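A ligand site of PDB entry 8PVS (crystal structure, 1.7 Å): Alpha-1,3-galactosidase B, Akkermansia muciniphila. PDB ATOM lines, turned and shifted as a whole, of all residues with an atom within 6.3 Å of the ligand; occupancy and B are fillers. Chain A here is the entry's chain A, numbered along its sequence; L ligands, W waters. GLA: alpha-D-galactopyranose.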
ATOM      1  N   ASN A 213       2.776  20.745  10.392  1.00  0.00           N
ATOM      2  CA  ASN A 213       2.463  19.370   9.969  1.00  0.00           C
ATOM      3  C   ASN A 213       2.456  18.390  11.135  1.00  0.00           C
ATOM      4  O   ASN A 213       2.767  17.209  10.960  1.00  0.00           O
ATOM      5  CB  ASN A 213       3.405  18.891   8.858  1.00  0.00           C
ATOM      6  CG  ASN A 213       3.164  19.604   7.537  1.00  0.00           C
ATOM      7  OD1 ASN A 213       3.329  20.827   7.435  1.00  0.00           O
ATOM      8  ND2 ASN A 213       2.752  18.851   6.510  1.00  0.00           N
ATOM      9  N   HIS A 214       2.070  18.876  12.325  1.00  0.00           N
ATOM     10  CA  HIS A 214       1.986  18.068  13.535  1.00  0.00           C
ATOM     11  C   HIS A 214       0.694  18.401  14.259  1.00  0.00           C
ATOM     12  O   HIS A 214       0.043  19.401  13.963  1.00  0.00           O
ATOM     13  CB  HIS A 214       3.208  18.285  14.435  1.00  0.00           C
ATOM     14  CG  HIS A 214       4.399  17.510  13.974  1.00  0.00           C
ATOM     15  ND1 HIS A 214       5.141  17.868  12.859  1.00  0.00           N
ATOM     16  CD2 HIS A 214       4.914  16.327  14.404  1.00  0.00           C
ATOM     17  CE1 HIS A 214       6.091  16.967  12.664  1.00  0.00           C
ATOM     18  NE2 HIS A 214       5.966  16.021  13.582  1.00  0.00           N
ATOM     19  N   ARG A 372       0.552  12.735  16.307  1.00  0.00           N
ATOM     20  CA  ARG A 372       1.947  13.131  16.144  1.00  0.00           C
ATOM     21  C   ARG A 372       2.163  14.433  16.893  1.00  0.00           C
ATOM     22  O   ARG A 372       2.216  15.509  16.305  1.00  0.00           O
ATOM     23  CB  ARG A 372       2.293  13.294  14.658  1.00  0.00           C
ATOM     24  CG  ARG A 372       1.148  13.938  13.811  1.00  0.00           C
ATOM     25  CD  ARG A 372       1.623  14.361  12.413  1.00  0.00           C
ATOM     26  NE  ARG A 372       1.835  13.226  11.508  1.00  0.00           N
ATOM     27  CZ  ARG A 372       2.163  13.343  10.224  1.00  0.00           C
ATOM     28  NH1 ARG A 372       2.434  14.525   9.685  1.00  0.00           N
ATOM     29  NH2 ARG A 372       2.204  12.247   9.469  1.00  0.00           N
ATOM     30  N   MET A 398       7.383  13.318  13.233  1.00  0.00           N
ATOM     31  CA  MET A 398       8.500  13.256  12.309  1.00  0.00           C
ATOM     32  C   MET A 398       9.803  13.235  13.097  1.00  0.00           C
ATOM     33  O   MET A 398       9.891  13.781  14.196  1.00  0.00           O
ATOM     34  CB  MET A 398       8.474  14.466  11.373  1.00  0.00           C
ATOM     35  CG  MET A 398       7.196  14.508  10.591  1.00  0.00           C
ATOM     36  SD  MET A 398       7.188  15.902   9.484  1.00  0.00           S
ATOM     37  CE  MET A 398       5.442  15.953   9.080  1.00  0.00           C
ATOM     38  N   ALA A 429       6.388   9.367  11.908  1.00  0.00           N
ATOM     39  CA  ALA A 429       5.964  10.010  10.666  1.00  0.00           C
ATOM     40  C   ALA A 429       7.182  10.166   9.754  1.00  0.00           C
ATOM     41  O   ALA A 429       8.037   9.262   9.713  1.00  0.00           O
ATOM     42  CB  ALA A 429       5.279  11.353  10.952  1.00  0.00           C
ATOM     43  N   ASP A 430       7.307  11.287   9.033  1.00  0.00           N
ATOM     44  CA  ASP A 430       8.408  11.457   8.079  1.00  0.00           C
ATOM     45  C   ASP A 430       9.760  11.331   8.771  1.00  0.00           C
ATOM     46  O   ASP A 430       9.908  11.634   9.950  1.00  0.00           O
ATOM     47  CB  ASP A 430       8.395  12.860   7.435  1.00  0.00           C
ATOM     48  CG  ASP A 430       7.044  13.285   6.933  1.00  0.00           C
ATOM     49  OD1 ASP A 430       6.012  12.982   7.581  1.00  0.00           O
ATOM     50  OD2 ASP A 430       7.029  13.987   5.894  1.00  0.00           O
ATOM     51  N   HIS A 433      11.608  16.703   7.004  1.00  0.00           N
ATOM     52  CA  HIS A 433      10.466  17.472   6.518  1.00  0.00           C
ATOM     53  C   HIS A 433      10.836  18.936   6.586  1.00  0.00           C
ATOM     54  O   HIS A 433      11.366  19.378   7.603  1.00  0.00           O
ATOM     55  CB  HIS A 433       9.243  17.175   7.375  1.00  0.00           C
ATOM     56  CG  HIS A 433       7.958  17.708   6.831  1.00  0.00           C
ATOM     57  ND1 HIS A 433       7.004  16.900   6.245  1.00  0.00           N
ATOM     58  CD2 HIS A 433       7.452  18.969   6.808  1.00  0.00           C
ATOM     59  CE1 HIS A 433       5.971  17.632   5.880  1.00  0.00           C
ATOM     60  NE2 HIS A 433       6.210  18.884   6.225  1.00  0.00           N
ATOM     61  N   ASP A 453       6.339   7.369   7.401  1.00  0.00           N
ATOM     62  CA  ASP A 453       6.023   8.228   6.275  1.00  0.00           C
ATOM     63  C   ASP A 453       7.252   8.429   5.401  1.00  0.00           C
ATOM     64  O   ASP A 453       8.177   7.603   5.459  1.00  0.00           O
ATOM     65  CB  ASP A 453       5.467   9.569   6.761  1.00  0.00           C
ATOM     66  CG  ASP A 453       4.361  10.086   5.852  1.00  0.00           C
ATOM     67  OD1 ASP A 453       4.640  10.320   4.658  1.00  0.00           O
ATOM     68  OD2 ASP A 453       3.219  10.243   6.332  1.00  0.00           O
ATOM     69  N   ASP A 454       7.289   9.483   4.604  1.00  0.00           N
ATOM     70  CA  ASP A 454       8.360   9.641   3.615  1.00  0.00           C
ATOM     71  C   ASP A 454       9.707   9.960   4.272  1.00  0.00           C
ATOM     72  O   ASP A 454       9.807  10.296   5.458  1.00  0.00           O
ATOM     73  CB  ASP A 454       8.007  10.727   2.605  1.00  0.00           C
ATOM     74  CG  ASP A 454       7.659  12.052   3.258  1.00  0.00           C
ATOM     75  OD1 ASP A 454       8.453  12.554   4.094  1.00  0.00           O
ATOM     76  OD2 ASP A 454       6.593  12.588   2.930  1.00  0.00           O
ATOM     77  N   ASN A 457      10.071  15.583   2.705  1.00  0.00           N
ATOM     78  CA  ASN A 457       8.967  16.315   2.085  1.00  0.00           C
ATOM     79  C   ASN A 457       9.328  17.789   2.204  1.00  0.00           C
ATOM     80  O   ASN A 457       9.485  18.290   3.318  1.00  0.00           O
ATOM     81  CB  ASN A 457       7.617  16.041   2.766  1.00  0.00           C
ATOM     82  CG  ASN A 457       6.472  16.885   2.195  1.00  0.00           C
ATOM     83  OD1 ASN A 457       6.651  17.714   1.292  1.00  0.00           O
ATOM     84  ND2 ASN A 457       5.265  16.646   2.704  1.00  0.00           N
ATOM     85  N   HIS A 459       8.090  21.598   1.096  1.00  0.00           N
ATOM     86  CA  HIS A 459       6.919  22.297   0.570  1.00  0.00           C
ATOM     87  C   HIS A 459       6.782  23.651   1.230  1.00  0.00           C
ATOM     88  O   HIS A 459       7.385  23.921   2.281  1.00  0.00           O
ATOM     89  CB  HIS A 459       5.653  21.484   0.825  1.00  0.00           C
ATOM     90  CG  HIS A 459       5.352  21.330   2.294  1.00  0.00           C
ATOM     91  ND1 HIS A 459       4.541  22.211   2.975  1.00  0.00           N
ATOM     92  CD2 HIS A 459       5.817  20.447   3.212  1.00  0.00           C
ATOM     93  CE1 HIS A 459       4.475  21.843   4.248  1.00  0.00           C
ATOM     94  NE2 HIS A 459       5.254  20.779   4.410  1.00  0.00           N
ATOM     95  N   GLN A 482      -3.287  20.688  11.081  1.00  0.00           N
ATOM     96  CA  GLN A 482      -1.960  20.388  11.594  1.00  0.00           C
ATOM     97  C   GLN A 482      -0.919  21.382  11.107  1.00  0.00           C
ATOM     98  O   GLN A 482       0.269  21.210  11.388  1.00  0.00           O
ATOM     99  CB  GLN A 482      -1.546  18.960  11.213  1.00  0.00           C
ATOM    100  CG  GLN A 482      -2.326  17.883  11.993  1.00  0.00           C
ATOM    101  CD  GLN A 482      -1.975  16.487  11.525  1.00  0.00           C
ATOM    102  OE1 GLN A 482      -1.803  16.243  10.326  1.00  0.00           O
ATOM    103  NE2 GLN A 482      -1.834  15.555  12.480  1.00  0.00           N
ATOM    104  N   ARG A 560       6.631   3.720   5.071  1.00  0.00           N
ATOM    105  CA  ARG A 560       5.227   3.931   4.759  1.00  0.00           C
ATOM    106  C   ARG A 560       5.069   5.061   3.756  1.00  0.00           C
ATOM    107  O   ARG A 560       5.818   6.054   3.781  1.00  0.00           O
ATOM    108  CB  ARG A 560       4.460   4.228   6.046  1.00  0.00           C
ATOM    109  CG  ARG A 560       2.957   4.411   5.843  1.00  0.00           C
ATOM    110  CD  ARG A 560       2.269   4.753   7.147  1.00  0.00           C
ATOM    111  NE  ARG A 560       0.957   5.283   6.828  1.00  0.00           N
ATOM    112  CZ  ARG A 560       0.748   6.498   6.342  1.00  0.00           C
ATOM    113  NH1 ARG A 560       1.750   7.363   6.177  1.00  0.00           N
ATOM    114  NH2 ARG A 560      -0.492   6.861   6.021  1.00  0.00           N
ATOM    115  N   ALA A 561       4.108   4.892   2.852  1.00  0.00           N
ATOM    116  CA  ALA A 561       3.775   5.896   1.866  1.00  0.00           C
ATOM    117  C   ALA A 561       4.967   6.115   0.940  1.00  0.00           C
ATOM    118  O   ALA A 561       5.722   5.166   0.637  1.00  0.00           O
ATOM    119  CB  ALA A 561       3.331   7.196   2.557  1.00  0.00           C
ATOM    120  N   ARG A 562       5.174   7.359   0.538  1.00  0.00           N
ATOM    121  CA  ARG A 562       6.110   7.662  -0.530  1.00  0.00           C
ATOM    122  C   ARG A 562       7.546   7.724  -0.020  1.00  0.00           C
ATOM    123  O   ARG A 562       7.819   7.950   1.156  1.00  0.00           O
ATOM    124  CB  ARG A 562       5.742   8.996  -1.202  1.00  0.00           C
ATOM    125  CG  ARG A 562       4.405   9.040  -1.928  1.00  0.00           C
ATOM    126  CD  ARG A 562       3.148   9.135  -1.006  1.00  0.00           C
ATOM    127  NE  ARG A 562       3.206  10.230  -0.046  1.00  0.00           N
ATOM    128  CZ  ARG A 562       2.215  11.093   0.171  1.00  0.00           C
ATOM    129  NH1 ARG A 562       1.081  11.026  -0.525  1.00  0.00           N
ATOM    130  NH2 ARG A 562       2.346  12.025   1.104  1.00  0.00           N
ATOM    131  N   LEU A 565       9.042  13.579  -1.354  1.00  0.00           N
ATOM    132  CA  LEU A 565       8.097  14.569  -1.890  1.00  0.00           C
ATOM    133  C   LEU A 565       8.807  15.901  -2.071  1.00  0.00           C
ATOM    134  O   LEU A 565       9.463  16.366  -1.142  1.00  0.00           O
ATOM    135  CB  LEU A 565       6.905  14.798  -0.931  1.00  0.00           C
ATOM    136  CG  LEU A 565       5.608  14.027  -1.082  1.00  0.00           C
ATOM    137  CD1 LEU A 565       5.819  12.555  -0.692  1.00  0.00           C
ATOM    138  CD2 LEU A 565       4.479  14.655  -0.235  1.00  0.00           C
ATOM    139  N   LEU A 588       7.314  11.825  -5.368  1.00  0.00           N
ATOM    140  CA  LEU A 588       6.054  12.500  -5.659  1.00  0.00           C
ATOM    141  C   LEU A 588       6.298  13.994  -5.736  1.00  0.00           C
ATOM    142  O   LEU A 588       6.874  14.589  -4.811  1.00  0.00           O
ATOM    143  CB  LEU A 588       4.994  12.190  -4.579  1.00  0.00           C
ATOM    144  CG  LEU A 588       3.739  13.076  -4.497  1.00  0.00           C
ATOM    145  CD1 LEU A 588       2.871  12.898  -5.731  1.00  0.00           C
ATOM    146  CD2 LEU A 588       2.911  12.750  -3.222  1.00  0.00           C
ATOM    147  N   ALA A 590       3.888  17.083  -5.747  1.00  0.00           N
ATOM    148  CA  ALA A 590       2.459  17.249  -5.469  1.00  0.00           C
ATOM    149  C   ALA A 590       2.079  18.723  -5.643  1.00  0.00           C
ATOM    150  O   ALA A 590       2.339  19.280  -6.722  1.00  0.00           O
ATOM    151  CB  ALA A 590       2.143  16.669  -4.094  1.00  0.00           C
ATOM    152  N   TRP A 596      -4.199  19.263   1.568  1.00  0.00           N
ATOM    153  CA  TRP A 596      -3.074  19.515   2.464  1.00  0.00           C
ATOM    154  C   TRP A 596      -2.678  20.987   2.500  1.00  0.00           C
ATOM    155  O   TRP A 596      -2.014  21.408   3.452  1.00  0.00           O
ATOM    156  CB  TRP A 596      -1.854  18.672   2.055  1.00  0.00           C
ATOM    157  CG  TRP A 596      -2.111  17.209   2.238  1.00  0.00           C
ATOM    158  CD1 TRP A 596      -2.486  16.312   1.271  1.00  0.00           C
ATOM    159  CD2 TRP A 596      -2.079  16.484   3.476  1.00  0.00           C
ATOM    160  NE1 TRP A 596      -2.650  15.061   1.822  1.00  0.00           N
ATOM    161  CE2 TRP A 596      -2.413  15.137   3.171  1.00  0.00           C
ATOM    162  CE3 TRP A 596      -1.755  16.822   4.800  1.00  0.00           C
ATOM    163  CZ2 TRP A 596      -2.440  14.131   4.151  1.00  0.00           C
ATOM    164  CZ3 TRP A 596      -1.781  15.816   5.780  1.00  0.00           C
ATOM    165  CH2 TRP A 596      -2.127  14.484   5.443  1.00  0.00           C
ATOM    166  N   GLU A 598      -0.426  22.374   0.670  1.00  0.00           N
ATOM    167  CA  GLU A 598       1.026  22.407   0.512  1.00  0.00           C
ATOM    168  C   GLU A 598       1.323  22.700  -0.938  1.00  0.00           C
ATOM    169  O   GLU A 598       0.777  22.033  -1.819  1.00  0.00           O
ATOM    170  CB  GLU A 598       1.659  21.075   0.906  1.00  0.00           C
ATOM    171  CG  GLU A 598       1.461  20.769   2.383  1.00  0.00           C
ATOM    172  CD  GLU A 598       2.081  19.442   2.806  1.00  0.00           C
ATOM    173  OE1 GLU A 598       2.804  18.801   1.995  1.00  0.00           O
ATOM    174  OE2 GLU A 598       1.822  19.035   3.956  1.00  0.00           O
ATOM    175  N   GLN A 621      -2.215   7.852  -1.038  1.00  0.00           N
ATOM    176  CA  GLN A 621      -2.681   9.013  -1.790  1.00  0.00           C
ATOM    177  C   GLN A 621      -1.631   9.415  -2.828  1.00  0.00           C
ATOM    178  O   GLN A 621      -0.437   9.516  -2.515  1.00  0.00           O
ATOM    179  CB  GLN A 621      -3.009  10.181  -0.858  1.00  0.00           C
ATOM    180  CG  GLN A 621      -3.820  11.288  -1.517  1.00  0.00           C
ATOM    181  CD  GLN A 621      -4.127  12.452  -0.579  1.00  0.00           C
ATOM    182  OE1 GLN A 621      -3.372  12.741   0.358  1.00  0.00           O
ATOM    183  NE2 GLN A 621      -5.236  13.137  -0.832  1.00  0.00           N
ATOM    184  N   PHE A 622      -2.089   9.612  -4.066  1.00  0.00           N
ATOM    185  CA  PHE A 622      -1.313  10.096  -5.216  1.00  0.00           C
ATOM    186  C   PHE A 622      -0.333   9.081  -5.816  1.00  0.00           C
ATOM    187  O   PHE A 622       0.466   9.458  -6.699  1.00  0.00           O
ATOM    188  CB  PHE A 622      -0.544  11.381  -4.880  1.00  0.00           C
ATOM    189  CG  PHE A 622      -1.405  12.471  -4.271  1.00  0.00           C
ATOM    190  CD1 PHE A 622      -2.574  12.887  -4.880  1.00  0.00           C
ATOM    191  CD2 PHE A 622      -1.000  13.084  -3.083  1.00  0.00           C
ATOM    192  CE1 PHE A 622      -3.352  13.895  -4.326  1.00  0.00           C
ATOM    193  CE2 PHE A 622      -1.780  14.084  -2.514  1.00  0.00           C
ATOM    194  CZ  PHE A 622      -2.958  14.490  -3.142  1.00  0.00           C
HETATM  195  C1  GLA L   1       3.019  13.221   4.668  1.00  0.00           C
HETATM  196  C2  GLA L   1       3.241  14.187   5.842  1.00  0.00           C
HETATM  197  C3  GLA L   1       2.074  15.106   5.982  1.00  0.00           C
HETATM  198  C4  GLA L   1       1.776  15.863   4.719  1.00  0.00           C
HETATM  199  C5  GLA L   1       1.545  14.874   3.578  1.00  0.00           C
HETATM  200  C6  GLA L   1       1.353  15.553   2.250  1.00  0.00           C
HETATM  201  O1  GLA L   1       2.002  12.338   4.908  1.00  0.00           O
HETATM  202  O2  GLA L   1       3.460  13.419   7.060  1.00  0.00           O
HETATM  203  O3  GLA L   1       2.281  16.058   7.069  1.00  0.00           O
HETATM  204  O4  GLA L   1       2.876  16.722   4.382  1.00  0.00           O
HETATM  205  O5  GLA L   1       2.684  13.963   3.427  1.00  0.00           O
HETATM  206  O6  GLA L   1       0.892  14.539   1.370  1.00  0.00           O
HETATM  207  O   HOH W   1      -0.261  10.038   5.603  1.00  0.00           O
HETATM  208  O   HOH W   2      -0.830  12.480   1.140  1.00  0.00           O
HETATM  209  O   HOH W   3       0.818  15.789  -0.923  1.00  0.00           O
HETATM  210  O   HOH W   4       0.247  17.131   8.412  1.00  0.00           O
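The side-chain carboxylate (OE2) of Glu 598 lies within hydrogen-bond range of an oxygen (O4) of the ligand, 2.6 Å away.
OD1 of Asp 430 lies within hydrogen-bond range of O2 of the ligand (2.6 Å).
The side-chain carboxylate of Asp 453 sits at hydrogen-bond distance from an oxygen (O1) of the ligand (2.8 Å).
An oxygen (O3) of the ligand lies within hydrogen-bond range of the side-chain amide nitrogen of Asn 213 (2.9 Å).
An oxygen (O6) of the ligand lies within hydrogen-bond range of the guanidinium group of Arg 562 (2.9 Å).
O4 of the ligand lies within hydrogen-bond range of ND2 of Asn 457, 2.9 Å away.
NH2 of Arg 372 lies within hydrogen-bond range of O2 of the ligand, at 3.0 Å.
Merely in contact with the ligand: Met 398, His 433, Leu 565 and Trp 596.
Hydrophobic or aromatic side chains within 4 Å of the ligand: Met 398, His 433, Leu 565 and Trp 596.
Within 4 Å of the ligand: Asn 213, Arg 372, Met 398, Asp 430, His 433, Asp 453, Asn 457, Arg 562, Leu 565, Trp 596 and Glu 598.
ND1 of His 433 sits at hydrogen-bond distance from OD2 of Asp 430, 2.9 Å away.
The side-chain carboxylate of Asp 453 lies within salt-bridge range of the guanidinium group of Arg 372 (3.9 Å).
The guanidinium group (NH1) of Arg 560 lies within salt-bridge range of the side-chain carboxylate (OD2) of Asp 453 (3.2 Å).
NH1 of Arg 372 is in hydrogen-bond range of O of Asn 213.
The side-chain amide nitrogen of Asn 213 sits close to a ring nitrogen (NE2) of His 433, 3.5 Å away.
The backbone NH (N) of Asn 213 sits at hydrogen-bond distance from the backbone carbonyl oxygen (O) of Gln 482, at 2.7 Å.
ND1 of His 433 sits close to SD of Met 398, 3.4 Å away.
The indole nitrogen (NE1) of Trp 596 sits at hydrogen-bond distance from the side-chain amide oxygen (OE1) of Gln 621 (2.8 Å).
Water W4 lies within hydrogen-bond range of O3 of the ligand (2.7 Å) and OE1 of Gln 482 (2.9 Å).
Water W2 lies within hydrogen-bond range of OE1 of Gln 621, O6 of the ligand, NH1 of Arg 562 and NE1 of Trp 596.
Water W1 lies within hydrogen-bond range of NH2 of Arg 560 (3.2 Å) and O1 of the ligand (3.3 Å).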
